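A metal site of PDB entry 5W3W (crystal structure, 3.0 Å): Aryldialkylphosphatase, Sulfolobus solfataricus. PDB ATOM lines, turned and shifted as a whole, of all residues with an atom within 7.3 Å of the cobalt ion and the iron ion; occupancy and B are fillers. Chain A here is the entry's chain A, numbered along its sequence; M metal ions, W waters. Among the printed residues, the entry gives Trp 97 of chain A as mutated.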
ATOM      1  N   HIS A  22      -5.364  -7.693  29.292  1.00  0.00           N
ATOM      2  CA  HIS A  22      -4.326  -6.706  29.046  1.00  0.00           C
ATOM      3  C   HIS A  22      -4.079  -5.929  30.355  1.00  0.00           C
ATOM      4  O   HIS A  22      -4.763  -4.957  30.689  1.00  0.00           O
ATOM      5  CB  HIS A  22      -4.767  -5.809  27.864  1.00  0.00           C
ATOM      6  CG  HIS A  22      -3.638  -5.039  27.249  1.00  0.00           C
ATOM      7  ND1 HIS A  22      -3.350  -5.091  25.900  1.00  0.00           N
ATOM      8  CD2 HIS A  22      -2.730  -4.201  27.796  1.00  0.00           C
ATOM      9  CE1 HIS A  22      -2.297  -4.337  25.646  1.00  0.00           C
ATOM     10  NE2 HIS A  22      -1.960  -3.692  26.755  1.00  0.00           N
ATOM     11  N   GLU A  23      -3.106  -6.370  31.123  1.00  0.00           N
ATOM     12  CA  GLU A  23      -2.630  -5.607  32.293  1.00  0.00           C
ATOM     13  C   GLU A  23      -1.085  -5.702  32.427  1.00  0.00           C
ATOM     14  O   GLU A  23      -0.461  -6.735  32.142  1.00  0.00           O
ATOM     15  CB  GLU A  23      -3.277  -6.103  33.566  1.00  0.00           C
ATOM     16  CG  GLU A  23      -4.783  -6.157  33.558  1.00  0.00           C
ATOM     17  CD  GLU A  23      -5.404  -4.794  33.567  1.00  0.00           C
ATOM     18  OE1 GLU A  23      -6.618  -4.710  33.285  1.00  0.00           O
ATOM     19  OE2 GLU A  23      -4.672  -3.823  33.852  1.00  0.00           O
ATOM     20  N   HIS A  24      -0.460  -4.616  32.853  1.00  0.00           N
ATOM     21  CA  HIS A  24       1.031  -4.565  32.946  1.00  0.00           C
ATOM     22  C   HIS A  24       1.423  -4.463  34.417  1.00  0.00           C
ATOM     23  O   HIS A  24       1.142  -3.458  35.101  1.00  0.00           O
ATOM     24  CB  HIS A  24       1.626  -3.354  32.190  1.00  0.00           C
ATOM     25  CG  HIS A  24       1.315  -3.322  30.712  1.00  0.00           C
ATOM     26  ND1 HIS A  24       2.123  -3.941  29.773  1.00  0.00           N
ATOM     27  CD2 HIS A  24       0.306  -2.723  30.023  1.00  0.00           C
ATOM     28  CE1 HIS A  24       1.594  -3.762  28.562  1.00  0.00           C
ATOM     29  NE2 HIS A  24       0.567  -2.916  28.681  1.00  0.00           N
ATOM     30  N   PRO A  67       1.063  -8.260  28.579  1.00  0.00           N
ATOM     31  CA  PRO A  67       1.697  -8.165  27.262  1.00  0.00           C
ATOM     32  C   PRO A  67       2.956  -7.266  27.242  1.00  0.00           C
ATOM     33  O   PRO A  67       3.317  -6.675  26.197  1.00  0.00           O
ATOM     34  CB  PRO A  67       0.555  -7.646  26.370  1.00  0.00           C
ATOM     35  CG  PRO A  67      -0.308  -6.871  27.279  1.00  0.00           C
ATOM     36  CD  PRO A  67      -0.071  -7.348  28.713  1.00  0.00           C
ATOM     37  N   THR A  68       3.667  -7.229  28.369  1.00  0.00           N
ATOM     38  CA  THR A  68       4.903  -6.507  28.496  1.00  0.00           C
ATOM     39  C   THR A  68       5.981  -7.303  27.757  1.00  0.00           C
ATOM     40  O   THR A  68       6.290  -8.422  28.153  1.00  0.00           O
ATOM     41  CB  THR A  68       5.300  -6.375  29.978  1.00  0.00           C
ATOM     42  OG1 THR A  68       4.261  -5.702  30.701  1.00  0.00           O
ATOM     43  CG2 THR A  68       6.517  -5.542  30.095  1.00  0.00           C
ATOM     44  N   LEU A  72       9.180  -2.542  26.497  1.00  0.00           N
ATOM     45  CA  LEU A  72       8.396  -2.264  27.674  1.00  0.00           C
ATOM     46  C   LEU A  72       9.014  -2.851  28.933  1.00  0.00           C
ATOM     47  O   LEU A  72       8.454  -2.739  30.023  1.00  0.00           O
ATOM     48  CB  LEU A  72       6.968  -2.816  27.475  1.00  0.00           C
ATOM     49  CG  LEU A  72       6.117  -2.181  26.328  1.00  0.00           C
ATOM     50  CD1 LEU A  72       4.807  -2.892  26.043  1.00  0.00           C
ATOM     51  CD2 LEU A  72       5.806  -0.731  26.659  1.00  0.00           C
ATOM     52  N   TRP A  97       7.760  -4.315  20.882  1.00  0.00           N
ATOM     53  CA  TRP A  97       6.984  -3.101  20.984  1.00  0.00           C
ATOM     54  C   TRP A  97       7.723  -1.903  20.362  1.00  0.00           C
ATOM     55  O   TRP A  97       8.584  -1.263  21.018  1.00  0.00           O
ATOM     56  CB  TRP A  97       6.702  -2.845  22.468  1.00  0.00           C
ATOM     57  CG  TRP A  97       5.535  -1.950  22.689  1.00  0.00           C
ATOM     58  CD1 TRP A  97       4.268  -2.319  22.755  1.00  0.00           C
ATOM     59  CD2 TRP A  97       5.558  -0.529  22.859  1.00  0.00           C
ATOM     60  NE1 TRP A  97       3.462  -1.246  22.956  1.00  0.00           N
ATOM     61  CE2 TRP A  97       4.220  -0.121  23.021  1.00  0.00           C
ATOM     62  CE3 TRP A  97       6.569   0.441  22.893  1.00  0.00           C
ATOM     63  CZ2 TRP A  97       3.838   1.201  23.245  1.00  0.00           C
ATOM     64  CZ3 TRP A  97       6.213   1.779  23.113  1.00  0.00           C
ATOM     65  CH2 TRP A  97       4.847   2.139  23.288  1.00  0.00           C
ATOM     66  N   TYR A  99       7.188   1.659  17.391  1.00  0.00           N
ATOM     67  CA  TYR A  99       6.337   2.518  16.545  1.00  0.00           C
ATOM     68  C   TYR A  99       6.923   2.814  15.180  1.00  0.00           C
ATOM     69  O   TYR A  99       6.195   2.861  14.194  1.00  0.00           O
ATOM     70  CB  TYR A  99       6.008   3.842  17.229  1.00  0.00           C
ATOM     71  CG  TYR A  99       5.168   3.718  18.473  1.00  0.00           C
ATOM     72  CD1 TYR A  99       4.397   2.553  18.735  1.00  0.00           C
ATOM     73  CD2 TYR A  99       5.069   4.773  19.359  1.00  0.00           C
ATOM     74  CE1 TYR A  99       3.605   2.453  19.868  1.00  0.00           C
ATOM     75  CE2 TYR A  99       4.275   4.682  20.493  1.00  0.00           C
ATOM     76  CZ  TYR A  99       3.538   3.537  20.740  1.00  0.00           C
ATOM     77  OH  TYR A  99       2.754   3.480  21.864  1.00  0.00           O
ATOM     78  N   KCX A 137       3.207 -10.362  21.184  1.00  0.00           N
ATOM     79  CA  KCX A 137       2.738  -8.978  21.134  1.00  0.00           C
ATOM     80  CB  KCX A 137       3.066  -8.257  22.464  1.00  0.00           C
ATOM     81  CG  KCX A 137       1.923  -7.307  22.889  1.00  0.00           C
ATOM     82  CD  KCX A 137       2.114  -5.930  22.317  1.00  0.00           C
ATOM     83  CE  KCX A 137       0.999  -5.029  22.773  1.00  0.00           C
ATOM     84  NZ  KCX A 137       1.216  -4.535  24.162  1.00  0.00           N
ATOM     85  C   KCX A 137       3.333  -8.142  20.037  1.00  0.00           C
ATOM     86  O   KCX A 137       4.531  -8.100  19.891  1.00  0.00           O
ATOM     87  CX  KCX A 137       0.622  -3.434  24.640  1.00  0.00           C
ATOM     88  OQ1 KCX A 137      -0.148  -2.781  23.958  1.00  0.00           O
ATOM     89  OQ2 KCX A 137       0.882  -3.118  25.855  1.00  0.00           O
ATOM     90  N   ILE A 138       2.501  -7.423  19.280  1.00  0.00           N
ATOM     91  CA  ILE A 138       3.004  -6.476  18.291  1.00  0.00           C
ATOM     92  C   ILE A 138       2.330  -5.112  18.464  1.00  0.00           C
ATOM     93  O   ILE A 138       1.324  -5.016  19.152  1.00  0.00           O
ATOM     94  CB  ILE A 138       2.891  -7.010  16.837  1.00  0.00           C
ATOM     95  CG1 ILE A 138       1.445  -7.176  16.380  1.00  0.00           C
ATOM     96  CG2 ILE A 138       3.631  -8.327  16.746  1.00  0.00           C
ATOM     97  CD1 ILE A 138       0.821  -5.899  15.854  1.00  0.00           C
ATOM     98  N   ALA A 139       2.880  -4.081  17.839  1.00  0.00           N
ATOM     99  CA  ALA A 139       2.354  -2.724  18.012  1.00  0.00           C
ATOM    100  C   ALA A 139       2.414  -1.915  16.704  1.00  0.00           C
ATOM    101  O   ALA A 139       2.978  -2.364  15.693  1.00  0.00           O
ATOM    102  CB  ALA A 139       3.083  -1.984  19.162  1.00  0.00           C
ATOM    103  N   ASP A 141       1.249   2.636  15.795  1.00  0.00           N
ATOM    104  CA  ASP A 141       0.646   3.838  16.362  1.00  0.00           C
ATOM    105  C   ASP A 141       0.699   4.956  15.321  1.00  0.00           C
ATOM    106  O   ASP A 141       0.706   4.645  14.145  1.00  0.00           O
ATOM    107  CB  ASP A 141       1.358   4.175  17.672  1.00  0.00           C
ATOM    108  CG  ASP A 141       0.489   4.955  18.613  1.00  0.00           C
ATOM    109  OD1 ASP A 141       0.079   6.084  18.197  1.00  0.00           O
ATOM    110  OD2 ASP A 141       0.221   4.469  19.739  1.00  0.00           O
ATOM    111  N   THR A 169      -2.317  -7.203  20.015  1.00  0.00           N
ATOM    112  CA  THR A 169      -1.702  -6.058  19.333  1.00  0.00           C
ATOM    113  C   THR A 169      -1.945  -4.783  20.079  1.00  0.00           C
ATOM    114  O   THR A 169      -2.831  -4.718  20.925  1.00  0.00           O
ATOM    115  CB  THR A 169      -2.199  -5.896  17.880  1.00  0.00           C
ATOM    116  OG1 THR A 169      -3.468  -5.248  17.891  1.00  0.00           O
ATOM    117  CG2 THR A 169      -2.263  -7.265  17.159  1.00  0.00           C
ATOM    118  N   HIS A 170      -1.137  -3.777  19.747  1.00  0.00           N
ATOM    119  CA  HIS A 170      -1.311  -2.379  20.180  1.00  0.00           C
ATOM    120  C   HIS A 170      -1.516  -1.522  18.918  1.00  0.00           C
ATOM    121  O   HIS A 170      -0.693  -1.528  17.976  1.00  0.00           O
ATOM    122  CB  HIS A 170      -0.103  -1.966  20.987  1.00  0.00           C
ATOM    123  CG  HIS A 170       0.053  -0.490  21.216  1.00  0.00           C
ATOM    124  ND1 HIS A 170      -0.052   0.067  22.480  1.00  0.00           N
ATOM    125  CD2 HIS A 170       0.265   0.542  20.352  1.00  0.00           C
ATOM    126  CE1 HIS A 170       0.225   1.360  22.376  1.00  0.00           C
ATOM    127  NE2 HIS A 170       0.381   1.682  21.098  1.00  0.00           N
ATOM    128  N   SER A 171      -2.616  -0.798  18.870  1.00  0.00           N
ATOM    129  CA  SER A 171      -2.951  -0.031  17.689  1.00  0.00           C
ATOM    130  C   SER A 171      -3.446   1.337  18.103  1.00  0.00           C
ATOM    131  O   SER A 171      -3.704   1.592  19.265  1.00  0.00           O
ATOM    132  CB  SER A 171      -3.983  -0.788  16.804  1.00  0.00           C
ATOM    133  OG  SER A 171      -5.237  -0.982  17.462  1.00  0.00           O
ATOM    134  N   GLY A 198      -6.054  -4.472  19.789  1.00  0.00           N
ATOM    135  CA  GLY A 198      -6.224  -3.743  21.046  1.00  0.00           C
ATOM    136  C   GLY A 198      -6.239  -2.243  20.891  1.00  0.00           C
ATOM    137  O   GLY A 198      -5.925  -1.673  19.844  1.00  0.00           O
ATOM    138  N   HIS A 199      -6.692  -1.641  21.972  1.00  0.00           N
ATOM    139  CA  HIS A 199      -6.814  -0.191  22.133  1.00  0.00           C
ATOM    140  C   HIS A 199      -7.867   0.468  21.283  1.00  0.00           C
ATOM    141  O   HIS A 199      -7.940   1.708  21.205  1.00  0.00           O
ATOM    142  CB  HIS A 199      -5.457   0.508  21.978  1.00  0.00           C
ATOM    143  CG  HIS A 199      -4.376  -0.111  22.804  1.00  0.00           C
ATOM    144  ND1 HIS A 199      -4.551  -0.485  24.133  1.00  0.00           N
ATOM    145  CD2 HIS A 199      -3.098  -0.433  22.485  1.00  0.00           C
ATOM    146  CE1 HIS A 199      -3.418  -0.998  24.587  1.00  0.00           C
ATOM    147  NE2 HIS A 199      -2.506  -0.911  23.633  1.00  0.00           N
ATOM    148  N   ASP A 222      -9.734  -2.151  25.962  1.00  0.00           N
ATOM    149  CA  ASP A 222      -8.757  -2.589  26.985  1.00  0.00           C
ATOM    150  C   ASP A 222      -8.059  -1.471  27.736  1.00  0.00           C
ATOM    151  O   ASP A 222      -7.147  -1.745  28.454  1.00  0.00           O
ATOM    152  CB  ASP A 222      -7.688  -3.467  26.314  1.00  0.00           C
ATOM    153  CG  ASP A 222      -7.167  -2.818  25.077  1.00  0.00           C
ATOM    154  OD1 ASP A 222      -7.337  -1.591  25.018  1.00  0.00           O
ATOM    155  OD2 ASP A 222      -6.683  -3.480  24.139  1.00  0.00           O
ATOM    156  N   ARG A 223      -8.498  -0.226  27.609  1.00  0.00           N
ATOM    157  CA  ARG A 223      -7.885   0.894  28.356  1.00  0.00           C
ATOM    158  C   ARG A 223      -8.876   1.648  29.279  1.00  0.00           C
ATOM    159  O   ARG A 223      -8.943   2.908  29.313  1.00  0.00           O
ATOM    160  CB  ARG A 223      -7.282   1.855  27.358  1.00  0.00           C
ATOM    161  CG  ARG A 223      -5.958   1.383  26.806  1.00  0.00           C
ATOM    162  CD  ARG A 223      -5.445   2.407  25.799  1.00  0.00           C
ATOM    163  NE  ARG A 223      -4.028   2.184  25.521  1.00  0.00           N
ATOM    164  CZ  ARG A 223      -3.335   2.760  24.551  1.00  0.00           C
ATOM    165  NH1 ARG A 223      -3.896   3.642  23.720  1.00  0.00           N
ATOM    166  NH2 ARG A 223      -2.054   2.429  24.405  1.00  0.00           N
ATOM    167  N   HIS A 255      -7.863  -2.925  31.382  1.00  0.00           N
ATOM    168  CA  HIS A 255      -7.489  -1.611  31.833  1.00  0.00           C
ATOM    169  C   HIS A 255      -6.240  -1.084  31.147  1.00  0.00           C
ATOM    170  O   HIS A 255      -6.160   0.156  30.926  1.00  0.00           O
ATOM    171  CB  HIS A 255      -7.251  -1.621  33.338  1.00  0.00           C
ATOM    172  CG  HIS A 255      -8.413  -2.138  34.120  1.00  0.00           C
ATOM    173  ND1 HIS A 255      -8.605  -3.475  34.336  1.00  0.00           N
ATOM    174  CD2 HIS A 255      -9.459  -1.503  34.698  1.00  0.00           C
ATOM    175  CE1 HIS A 255      -9.708  -3.643  35.058  1.00  0.00           C
ATOM    176  NE2 HIS A 255     -10.232  -2.457  35.291  1.00  0.00           N
ATOM    177  N   ASP A 256      -5.291  -1.977  30.827  1.00  0.00           N
ATOM    178  CA  ASP A 256      -3.933  -1.597  30.303  1.00  0.00           C
ATOM    179  C   ASP A 256      -3.174  -0.830  31.366  1.00  0.00           C
ATOM    180  O   ASP A 256      -2.337   0.003  31.069  1.00  0.00           O
ATOM    181  CB  ASP A 256      -4.009  -0.797  28.981  1.00  0.00           C
ATOM    182  CG  ASP A 256      -2.664  -0.705  28.226  1.00  0.00           C
ATOM    183  OD1 ASP A 256      -1.743  -1.464  28.503  1.00  0.00           O
ATOM    184  OD2 ASP A 256      -2.508   0.143  27.321  1.00  0.00           O
ATOM    185  N   TYR A 257      -3.474  -1.141  32.612  1.00  0.00           N
ATOM    186  CA  TYR A 257      -2.900  -0.456  33.758  1.00  0.00           C
ATOM    187  C   TYR A 257      -1.421  -0.831  33.948  1.00  0.00           C
ATOM    188  O   TYR A 257      -1.022  -1.958  33.681  1.00  0.00           O
ATOM    189  CB  TYR A 257      -3.700  -0.778  35.001  1.00  0.00           C
ATOM    190  CG  TYR A 257      -3.270  -0.033  36.241  1.00  0.00           C
ATOM    191  CD1 TYR A 257      -3.506   1.344  36.368  1.00  0.00           C
ATOM    192  CD2 TYR A 257      -2.667  -0.695  37.313  1.00  0.00           C
ATOM    193  CE1 TYR A 257      -3.120   2.036  37.522  1.00  0.00           C
ATOM    194  CE2 TYR A 257      -2.279  -0.013  38.466  1.00  0.00           C
ATOM    195  CZ  TYR A 257      -2.516   1.355  38.572  1.00  0.00           C
ATOM    196  OH  TYR A 257      -2.146   2.047  39.698  1.00  0.00           O
ATOM    197  N   CYS A 258      -0.651   0.161  34.410  1.00  0.00           N
ATOM    198  CA  CYS A 258       0.788   0.038  34.665  1.00  0.00           C
ATOM    199  C   CYS A 258       1.083   0.420  36.103  1.00  0.00           C
ATOM    200  O   CYS A 258       1.230   1.616  36.417  1.00  0.00           O
ATOM    201  CB  CYS A 258       1.589   0.982  33.759  1.00  0.00           C
ATOM    202  SG  CYS A 258       1.153   0.975  32.006  1.00  0.00           S
HETATM  203 CO    CO M   1      -0.615  -0.961  24.171  1.00  0.00          CO
HETATM  204 FE    FE M   2      -0.472  -2.252  27.062  1.00  0.00          FE
HETATM  205  O   HOH W   1       0.165  -0.171  26.457  1.00  0.00           O
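The cobalt ion is bound by OQ1 of KCX 137 (1.9 Å), a ring nitrogen (NE2) of His 199 (2.0 Å), a ring nitrogen (ND1) of His 170 (2.1 Å) and water W1 (2.5 Å).
Residues that only touch the cobalt ion: Arg 223 (3.7 Å).
Within 4 Å of the cobalt ion: His 22, KCX 137, His 170, His 199, Arg 223 and Asp 256.
Along chain A the residues within 4 Å of the cobalt ion span positions 22 to 256.
The nearest printed residue that does not touch the iron ion is His 199 (4.05 Å).
N of Asp 256 sits at hydrogen-bond distance from O of Asp 222.
SG of Cys 258 lies within hydrogen-bond range of O of Asp 256 (3.7 Å).
The backbone carbonyl oxygen (O) of Tyr 257 sits at hydrogen-bond distance from the backbone NH (N) of His 24.
NE of Arg 223 is in salt-bridge range of OD2 of Asp 256, 3.1 Å away.
A ring nitrogen (ND1) of His 24 sits at hydrogen-bond distance from the side-chain hydroxyl of Thr 68, 2.9 Å away.
OD2 of Asp 141 sits at hydrogen-bond distance from NE2 of His 170 (3.1 Å).
The backbone NH (N) of His 170 sits at hydrogen-bond distance from the backbone carbonyl oxygen (O) of Ile 138, 2.8 Å away.
The backbone NH (N) of His 199 is in hydrogen-bond range of the side-chain carboxylate (OD2) of Asp 222 (2.8 Å).
OQ2 of KCX 137 binds the iron ion, at 2.0 Å.
The iron ion is bound by NE2 of His 24.
The iron ion is bound by OD1 of Asp 256 (2.1 Å).
NE2 of His 22 binds the iron ion (2.1 Å).
The iron ion is bound by water W1 (2.3 Å).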
